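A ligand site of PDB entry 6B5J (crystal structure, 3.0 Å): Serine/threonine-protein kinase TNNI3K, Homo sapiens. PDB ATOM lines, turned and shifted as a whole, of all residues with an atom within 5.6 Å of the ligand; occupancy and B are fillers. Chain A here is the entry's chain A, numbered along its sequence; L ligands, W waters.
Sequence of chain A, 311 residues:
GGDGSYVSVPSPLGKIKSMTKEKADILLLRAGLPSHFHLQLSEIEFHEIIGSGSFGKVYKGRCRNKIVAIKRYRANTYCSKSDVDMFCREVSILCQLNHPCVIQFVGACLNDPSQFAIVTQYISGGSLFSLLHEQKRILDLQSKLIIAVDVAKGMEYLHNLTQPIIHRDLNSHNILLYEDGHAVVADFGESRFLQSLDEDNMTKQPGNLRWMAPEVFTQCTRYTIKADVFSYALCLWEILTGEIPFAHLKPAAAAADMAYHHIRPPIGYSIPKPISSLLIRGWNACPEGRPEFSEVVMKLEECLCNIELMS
Residues that only touch the ligand: Ile 50, Val 58, Ala 69, Lys 71, Ile 103, Gln 121, Tyr 122, Ser 124, Gly 126, Leu 176 and Ala 186. Hydrophobic or aromatic side chains that line the ligand: Ile 50, Val 58, Ala 69, Ile 103, Tyr 122, Ile 123, Leu 176 and Ala 186. Within 4 Å of the ligand: Ile 50, Val 58, Ala 69, Lys 71, Ile 103, Thr 120, Gln 121, Tyr 122, Ile 123, Ser 124, Gly 126, Leu 176, Ala 186 and Asp 187. The nearest printed residue that does not touch the ligand is Ile 118 (4.01 Å).
The side-chain hydroxyl (OG1) of Thr 120 is in hydrogen-bond range of a nitrogen (N1) of the ligand. An oxygen (O2) of the ligand sits at hydrogen-bond distance from the backbone NH of Asp 187 (3.0 Å). The backbone NH of Ile 123 is in hydrogen-bond range of a nitrogen (N4) of the ligand (2.9 Å). O of Ile 123 sits at hydrogen-bond distance from N3 of the ligand, at 2.5 Å.
The side-chain carboxylate (OD1) of Asp 187 is in salt-bridge range of the side-chain amino group (NZ) of Lys 71 (2.9 Å). The backbone carbonyl oxygen of Thr 120 is in hydrogen-bond range of the backbone NH of Ala 69 (2.9 Å). The side-chain amino group (NZ) of Lys 71 is in salt-bridge range of the side-chain carboxylate (OE2) of Glu 90. The backbone carbonyl oxygen (O) of Asn 174 sits at hydrogen-bond distance from the backbone NH (N) of Ala 186. O of Val 58 lies within hydrogen-bond range of N of Ile 50, 2.9 Å away. The backbone NH (N) of Lys 71 sits at hydrogen-bond distance from the backbone carbonyl oxygen (O) of Ile 118, at 2.8 Å.
Water W1 lies within hydrogen-bond range of O1 of the ligand (2.7 Å), OE2 of Glu 90 (2.9 Å) and N of Phe 188 (2.9 Å).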
ATOM      1  N   ILE A  50      12.651 -21.564 -27.259  1.00  0.00           N
ATOM      2  CA  ILE A  50      12.133 -21.598 -25.857  1.00  0.00           C
ATOM      3  C   ILE A  50      11.707 -20.247 -25.289  1.00  0.00           C
ATOM      4  O   ILE A  50      10.960 -20.210 -24.317  1.00  0.00           O
ATOM      5  CB  ILE A  50      13.074 -22.346 -24.861  1.00  0.00           C
ATOM      6  CG1 ILE A  50      14.541 -21.928 -25.075  1.00  0.00           C
ATOM      7  CG2 ILE A  50      12.886 -23.866 -25.004  1.00  0.00           C
ATOM      8  CD1 ILE A  50      15.574 -22.677 -24.250  1.00  0.00           C
ATOM      9  N   VAL A  58      15.665 -17.076 -28.150  1.00  0.00           N
ATOM     10  CA  VAL A  58      16.420 -18.050 -27.378  1.00  0.00           C
ATOM     11  C   VAL A  58      16.074 -19.460 -27.841  1.00  0.00           C
ATOM     12  O   VAL A  58      14.906 -19.877 -27.822  1.00  0.00           O
ATOM     13  CB  VAL A  58      16.115 -17.927 -25.860  1.00  0.00           C
ATOM     14  CG1 VAL A  58      16.862 -19.011 -25.080  1.00  0.00           C
ATOM     15  CG2 VAL A  58      16.494 -16.543 -25.326  1.00  0.00           C
ATOM     16  N   ALA A  69      21.374 -23.704 -24.113  1.00  0.00           N
ATOM     17  CA  ALA A  69      20.420 -22.688 -24.490  1.00  0.00           C
ATOM     18  C   ALA A  69      21.201 -21.612 -25.192  1.00  0.00           C
ATOM     19  O   ALA A  69      22.274 -21.256 -24.728  1.00  0.00           O
ATOM     20  CB  ALA A  69      19.763 -22.132 -23.260  1.00  0.00           C
ATOM     21  N   ILE A  70      20.664 -21.101 -26.291  1.00  0.00           N
ATOM     22  CA  ILE A  70      21.351 -20.090 -27.088  1.00  0.00           C
ATOM     23  C   ILE A  70      20.494 -18.876 -27.232  1.00  0.00           C
ATOM     24  O   ILE A  70      19.409 -18.961 -27.782  1.00  0.00           O
ATOM     25  CB  ILE A  70      21.673 -20.562 -28.531  1.00  0.00           C
ATOM     26  CG1 ILE A  70      22.397 -21.918 -28.530  1.00  0.00           C
ATOM     27  CG2 ILE A  70      22.495 -19.497 -29.287  1.00  0.00           C
ATOM     28  CD1 ILE A  70      21.510 -23.074 -28.912  1.00  0.00           C
ATOM     29  N   LYS A  71      21.014 -17.729 -26.832  1.00  0.00           N
ATOM     30  CA  LYS A  71      20.320 -16.469 -27.007  1.00  0.00           C
ATOM     31  C   LYS A  71      20.922 -15.830 -28.229  1.00  0.00           C
ATOM     32  O   LYS A  71      22.096 -15.498 -28.229  1.00  0.00           O
ATOM     33  CB  LYS A  71      20.511 -15.552 -25.784  1.00  0.00           C
ATOM     34  CG  LYS A  71      19.983 -14.134 -25.926  1.00  0.00           C
ATOM     35  CD  LYS A  71      20.572 -13.208 -24.874  1.00  0.00           C
ATOM     36  CE  LYS A  71      19.787 -13.200 -23.573  1.00  0.00           C
ATOM     37  NZ  LYS A  71      19.759 -11.847 -22.915  1.00  0.00           N
ATOM     38  N   GLU A  90      27.178  -7.755 -21.964  1.00  0.00           N
ATOM     39  CA  GLU A  90      26.600  -8.997 -21.503  1.00  0.00           C
ATOM     40  C   GLU A  90      27.629 -10.096 -21.449  1.00  0.00           C
ATOM     41  O   GLU A  90      27.653 -10.861 -20.485  1.00  0.00           O
ATOM     42  CB  GLU A  90      25.410  -9.448 -22.374  1.00  0.00           C
ATOM     43  CG  GLU A  90      24.718 -10.735 -21.859  1.00  0.00           C
ATOM     44  CD  GLU A  90      23.377 -11.075 -22.536  1.00  0.00           C
ATOM     45  OE1 GLU A  90      23.029 -10.390 -23.490  1.00  0.00           O
ATOM     46  OE2 GLU A  90      22.669 -12.034 -22.133  1.00  0.00           O
ATOM     47  N   LEU A  94      29.024 -12.194 -18.318  1.00  0.00           N
ATOM     48  CA  LEU A  94      28.850 -13.653 -18.273  1.00  0.00           C
ATOM     49  C   LEU A  94      30.144 -14.414 -18.107  1.00  0.00           C
ATOM     50  O   LEU A  94      30.214 -15.369 -17.352  1.00  0.00           O
ATOM     51  CB  LEU A  94      28.144 -14.181 -19.522  1.00  0.00           C
ATOM     52  CG  LEU A  94      26.623 -14.084 -19.525  1.00  0.00           C
ATOM     53  CD1 LEU A  94      26.112 -14.325 -20.936  1.00  0.00           C
ATOM     54  CD2 LEU A  94      26.000 -15.088 -18.574  1.00  0.00           C
ATOM     55  N   ILE A 103      23.476 -19.406 -13.754  1.00  0.00           N
ATOM     56  CA  ILE A 103      23.552 -20.074 -15.062  1.00  0.00           C
ATOM     57  C   ILE A 103      24.969 -20.127 -15.589  1.00  0.00           C
ATOM     58  O   ILE A 103      25.639 -19.129 -15.598  1.00  0.00           O
ATOM     59  CB  ILE A 103      22.636 -19.386 -16.137  1.00  0.00           C
ATOM     60  CG1 ILE A 103      22.318 -20.348 -17.265  1.00  0.00           C
ATOM     61  CG2 ILE A 103      23.278 -18.138 -16.792  1.00  0.00           C
ATOM     62  CD1 ILE A 103      21.507 -21.537 -16.814  1.00  0.00           C
ATOM     63  N   ILE A 118      24.887 -15.822 -27.614  1.00  0.00           N
ATOM     64  CA  ILE A 118      25.327 -16.233 -26.319  1.00  0.00           C
ATOM     65  C   ILE A 118      24.849 -17.672 -26.030  1.00  0.00           C
ATOM     66  O   ILE A 118      23.707 -18.003 -26.243  1.00  0.00           O
ATOM     67  CB  ILE A 118      24.812 -15.231 -25.309  1.00  0.00           C
ATOM     68  CG1 ILE A 118      25.715 -14.004 -25.368  1.00  0.00           C
ATOM     69  CG2 ILE A 118      24.819 -15.788 -23.903  1.00  0.00           C
ATOM     70  CD1 ILE A 118      25.122 -12.756 -24.717  1.00  0.00           C
ATOM     71  N   VAL A 119      25.759 -18.505 -25.531  1.00  0.00           N
ATOM     72  CA  VAL A 119      25.484 -19.907 -25.230  1.00  0.00           C
ATOM     73  C   VAL A 119      25.715 -20.232 -23.752  1.00  0.00           C
ATOM     74  O   VAL A 119      26.777 -19.959 -23.214  1.00  0.00           O
ATOM     75  CB  VAL A 119      26.365 -20.808 -26.119  1.00  0.00           C
ATOM     76  CG1 VAL A 119      25.893 -22.254 -26.028  1.00  0.00           C
ATOM     77  CG2 VAL A 119      26.328 -20.340 -27.569  1.00  0.00           C
ATOM     78  N   THR A 120      24.709 -20.802 -23.090  1.00  0.00           N
ATOM     79  CA  THR A 120      24.815 -21.249 -21.708  1.00  0.00           C
ATOM     80  C   THR A 120      24.358 -22.693 -21.619  1.00  0.00           C
ATOM     81  O   THR A 120      23.814 -23.215 -22.564  1.00  0.00           O
ATOM     82  CB  THR A 120      23.888 -20.444 -20.778  1.00  0.00           C
ATOM     83  OG1 THR A 120      22.503 -20.703 -21.130  1.00  0.00           O
ATOM     84  CG2 THR A 120      24.234 -18.948 -20.852  1.00  0.00           C
ATOM     85  N   GLN A 121      24.535 -23.297 -20.447  1.00  0.00           N
ATOM     86  CA  GLN A 121      23.890 -24.569 -20.141  1.00  0.00           C
ATOM     87  C   GLN A 121      22.375 -24.425 -20.323  1.00  0.00           C
ATOM     88  O   GLN A 121      21.815 -23.325 -20.272  1.00  0.00           O
ATOM     89  CB  GLN A 121      24.208 -25.057 -18.712  1.00  0.00           C
ATOM     90  CG  GLN A 121      23.477 -24.273 -17.601  1.00  0.00           C
ATOM     91  CD  GLN A 121      23.829 -24.673 -16.142  1.00  0.00           C
ATOM     92  OE1 GLN A 121      24.197 -23.802 -15.322  1.00  0.00           O
ATOM     93  NE2 GLN A 121      23.629 -25.958 -15.805  1.00  0.00           N
ATOM     94  N   TYR A 122      21.758 -25.572 -20.538  1.00  0.00           N
ATOM     95  CA  TYR A 122      20.318 -25.743 -20.605  1.00  0.00           C
ATOM     96  C   TYR A 122      19.872 -26.477 -19.353  1.00  0.00           C
ATOM     97  O   TYR A 122      20.461 -27.465 -18.997  1.00  0.00           O
ATOM     98  CB  TYR A 122      19.924 -26.574 -21.813  1.00  0.00           C
ATOM     99  CG  TYR A 122      18.458 -26.926 -21.920  1.00  0.00           C
ATOM    100  CD1 TYR A 122      17.537 -25.995 -22.418  1.00  0.00           C
ATOM    101  CD2 TYR A 122      17.991 -28.198 -21.594  1.00  0.00           C
ATOM    102  CE1 TYR A 122      16.187 -26.307 -22.571  1.00  0.00           C
ATOM    103  CE2 TYR A 122      16.647 -28.531 -21.738  1.00  0.00           C
ATOM    104  CZ  TYR A 122      15.749 -27.585 -22.221  1.00  0.00           C
ATOM    105  OH  TYR A 122      14.416 -27.912 -22.376  1.00  0.00           O
ATOM    106  N   ILE A 123      18.839 -25.961 -18.709  1.00  0.00           N
ATOM    107  CA  ILE A 123      18.330 -26.482 -17.468  1.00  0.00           C
ATOM    108  C   ILE A 123      16.972 -27.057 -17.787  1.00  0.00           C
ATOM    109  O   ILE A 123      16.075 -26.349 -18.256  1.00  0.00           O
ATOM    110  CB  ILE A 123      18.244 -25.346 -16.466  1.00  0.00           C
ATOM    111  CG1 ILE A 123      19.646 -24.741 -16.297  1.00  0.00           C
ATOM    112  CG2 ILE A 123      17.606 -25.851 -15.177  1.00  0.00           C
ATOM    113  CD1 ILE A 123      20.176 -24.667 -14.884  1.00  0.00           C
ATOM    114  N   SER A 124      16.825 -28.365 -17.552  1.00  0.00           N
ATOM    115  CA  SER A 124      15.724 -29.125 -18.140  1.00  0.00           C
ATOM    116  C   SER A 124      14.421 -28.911 -17.417  1.00  0.00           C
ATOM    117  O   SER A 124      13.341 -29.153 -17.991  1.00  0.00           O
ATOM    118  CB  SER A 124      16.041 -30.629 -18.204  1.00  0.00           C
ATOM    119  OG  SER A 124      15.742 -31.264 -16.960  1.00  0.00           O
ATOM    120  N   GLY A 125      14.525 -28.515 -16.156  1.00  0.00           N
ATOM    121  CA  GLY A 125      13.321 -28.428 -15.346  1.00  0.00           C
ATOM    122  C   GLY A 125      12.526 -27.144 -15.502  1.00  0.00           C
ATOM    123  O   GLY A 125      11.487 -26.972 -14.857  1.00  0.00           O
ATOM    124  N   GLY A 126      13.024 -26.228 -16.312  1.00  0.00           N
ATOM    125  CA  GLY A 126      12.274 -25.045 -16.673  1.00  0.00           C
ATOM    126  C   GLY A 126      12.384 -23.854 -15.744  1.00  0.00           C
ATOM    127  O   GLY A 126      13.186 -23.831 -14.800  1.00  0.00           O
ATOM    128  N   SER A 127      11.519 -22.867 -16.033  1.00  0.00           N
ATOM    129  CA  SER A 127      11.472 -21.643 -15.266  1.00  0.00           C
ATOM    130  C   SER A 127      10.531 -21.825 -14.068  1.00  0.00           C
ATOM    131  O   SER A 127       9.593 -22.666 -14.105  1.00  0.00           O
ATOM    132  CB  SER A 127      11.058 -20.435 -16.129  1.00  0.00           C
ATOM    133  OG  SER A 127       9.661 -20.329 -16.391  1.00  0.00           O
ATOM    134  N   SER A 130       6.960 -20.950 -15.028  1.00  0.00           N
ATOM    135  CA  SER A 130       6.241 -22.114 -15.572  1.00  0.00           C
ATOM    136  C   SER A 130       5.752 -23.075 -14.491  1.00  0.00           C
ATOM    137  O   SER A 130       4.589 -23.435 -14.486  1.00  0.00           O
ATOM    138  CB  SER A 130       7.104 -22.884 -16.545  1.00  0.00           C
ATOM    139  OG  SER A 130       7.564 -22.020 -17.544  1.00  0.00           O
ATOM    140  N   GLN A 135       2.194 -24.852 -15.186  1.00  0.00           N
ATOM    141  CA  GLN A 135       1.990 -26.189 -14.663  1.00  0.00           C
ATOM    142  C   GLN A 135       1.338 -26.186 -13.260  1.00  0.00           C
ATOM    143  O   GLN A 135       1.005 -27.237 -12.757  1.00  0.00           O
ATOM    144  CB  GLN A 135       3.318 -26.943 -14.635  1.00  0.00           C
ATOM    145  CG  GLN A 135       3.980 -27.024 -16.003  1.00  0.00           C
ATOM    146  CD  GLN A 135       5.492 -27.186 -15.904  1.00  0.00           C
ATOM    147  OE1 GLN A 135       6.170 -26.410 -15.243  1.00  0.00           O
ATOM    148  NE2 GLN A 135       6.016 -28.193 -16.584  1.00  0.00           N
ATOM    149  N   ASN A 174      13.417 -15.855 -14.975  1.00  0.00           N
ATOM    150  CA  ASN A 174      14.876 -15.987 -14.938  1.00  0.00           C
ATOM    151  C   ASN A 174      15.430 -16.808 -13.788  1.00  0.00           C
ATOM    152  O   ASN A 174      16.628 -16.887 -13.620  1.00  0.00           O
ATOM    153  CB  ASN A 174      15.449 -14.593 -14.862  1.00  0.00           C
ATOM    154  CG  ASN A 174      15.092 -13.763 -16.076  1.00  0.00           C
ATOM    155  OD1 ASN A 174      14.758 -14.310 -17.168  1.00  0.00           O
ATOM    156  ND2 ASN A 174      15.159 -12.432 -15.914  1.00  0.00           N
ATOM    157  N   LEU A 176      15.533 -20.556 -13.100  1.00  0.00           N
ATOM    158  CA  LEU A 176      15.408 -21.862 -13.733  1.00  0.00           C
ATOM    159  C   LEU A 176      15.702 -22.947 -12.726  1.00  0.00           C
ATOM    160  O   LEU A 176      16.346 -22.698 -11.697  1.00  0.00           O
ATOM    161  CB  LEU A 176      16.404 -21.957 -14.884  1.00  0.00           C
ATOM    162  CG  LEU A 176      16.382 -20.766 -15.860  1.00  0.00           C
ATOM    163  CD1 LEU A 176      17.418 -20.929 -16.966  1.00  0.00           C
ATOM    164  CD2 LEU A 176      15.008 -20.615 -16.449  1.00  0.00           C
ATOM    165  N   ALA A 186      19.357 -16.831 -14.165  1.00  0.00           N
ATOM    166  CA  ALA A 186      19.716 -16.811 -15.565  1.00  0.00           C
ATOM    167  C   ALA A 186      19.481 -15.453 -16.176  1.00  0.00           C
ATOM    168  O   ALA A 186      18.906 -14.591 -15.567  1.00  0.00           O
ATOM    169  CB  ALA A 186      18.909 -17.876 -16.289  1.00  0.00           C
ATOM    170  N   ASP A 187      19.929 -15.271 -17.397  1.00  0.00           N
ATOM    171  CA  ASP A 187      19.640 -14.090 -18.205  1.00  0.00           C
ATOM    172  C   ASP A 187      20.165 -12.780 -17.638  1.00  0.00           C
ATOM    173  O   ASP A 187      19.483 -12.080 -16.902  1.00  0.00           O
ATOM    174  CB  ASP A 187      18.171 -13.965 -18.579  1.00  0.00           C
ATOM    175  CG  ASP A 187      17.939 -13.049 -19.778  1.00  0.00           C
ATOM    176  OD1 ASP A 187      18.898 -12.407 -20.226  1.00  0.00           O
ATOM    177  OD2 ASP A 187      16.781 -12.946 -20.268  1.00  0.00           O
ATOM    178  N   PHE A 188      21.376 -12.460 -18.063  1.00  0.00           N
ATOM    179  CA  PHE A 188      22.084 -11.280 -17.686  1.00  0.00           C
ATOM    180  C   PHE A 188      21.963 -10.232 -18.779  1.00  0.00           C
ATOM    181  O   PHE A 188      22.895  -9.418 -18.973  1.00  0.00           O
ATOM    182  CB  PHE A 188      23.541 -11.662 -17.390  1.00  0.00           C
ATOM    183  CG  PHE A 188      23.651 -12.463 -16.159  1.00  0.00           C
ATOM    184  CD1 PHE A 188      23.242 -13.760 -16.141  1.00  0.00           C
ATOM    185  CD2 PHE A 188      24.067 -11.882 -14.975  1.00  0.00           C
ATOM    186  CE1 PHE A 188      23.267 -14.500 -14.969  1.00  0.00           C
ATOM    187  CE2 PHE A 188      24.117 -12.602 -13.810  1.00  0.00           C
ATOM    188  CZ  PHE A 188      23.706 -13.906 -13.808  1.00  0.00           C
HETATM  189  C1  LIG L   1      16.787 -18.630 -21.040  1.00  0.00           C
HETATM  190  C2  LIG L   1      15.777 -22.134 -20.385  1.00  0.00           C
HETATM  191  C3  LIG L   1      13.406 -23.883 -21.038  1.00  0.00           C
HETATM  192  C4  LIG L   1      12.415 -26.364 -20.392  1.00  0.00           C
HETATM  193  C5  LIG L   1      13.683 -25.999 -19.991  1.00  0.00           C
HETATM  194  C6  LIG L   1      10.252 -25.957 -21.536  1.00  0.00           C
HETATM  195  C7  LIG L   1      21.167 -18.178 -23.148  1.00  0.00           C
HETATM  196  N1  LIG L   1      21.078 -18.358 -21.694  1.00  0.00           N
HETATM  197  S1  LIG L   1      20.459 -17.039 -20.800  1.00  0.00           S
HETATM  198  O1  LIG L   1      20.858 -15.785 -21.429  1.00  0.00           O
HETATM  199  O2  LIG L   1      20.693 -17.359 -19.403  1.00  0.00           O
HETATM  200  C8  LIG L   1      18.728 -17.241 -21.041  1.00  0.00           C
HETATM  201  C9  LIG L   1      17.985 -16.131 -21.375  1.00  0.00           C
HETATM  202  C10 LIG L   1      16.625 -16.277 -21.559  1.00  0.00           C
HETATM  203  C11 LIG L   1      16.039 -17.510 -21.391  1.00  0.00           C
HETATM  204  N2  LIG L   1      16.092 -19.861 -20.899  1.00  0.00           N
HETATM  205  C12 LIG L   1      16.646 -21.084 -20.517  1.00  0.00           C
HETATM  206  C13 LIG L   1      16.308 -23.360 -20.011  1.00  0.00           C
HETATM  207  N3  LIG L   1      15.505 -24.499 -19.855  1.00  0.00           N
HETATM  208  C14 LIG L   1      14.190 -24.757 -20.310  1.00  0.00           C
HETATM  209  C15 LIG L   1      12.142 -24.236 -21.444  1.00  0.00           C
HETATM  210  C16 LIG L   1      11.630 -25.490 -21.119  1.00  0.00           C
HETATM  211  F1  LIG L   1       9.469 -26.320 -20.468  1.00  0.00           F
HETATM  212  F2  LIG L   1       9.547 -25.084 -22.334  1.00  0.00           F
HETATM  213  F3  LIG L   1      10.337 -27.072 -22.309  1.00  0.00           F
HETATM  214  N4  LIG L   1      17.613 -23.526 -19.769  1.00  0.00           N
HETATM  215  C17 LIG L   1      18.383 -22.439 -19.934  1.00  0.00           C
HETATM  216  N5  LIG L   1      17.958 -21.222 -20.297  1.00  0.00           N
HETATM  217  C18 LIG L   1      18.153 -18.477 -20.854  1.00  0.00           C
HETATM  218  O   HOH W   1      22.605 -14.115 -20.127  1.00  0.00           O
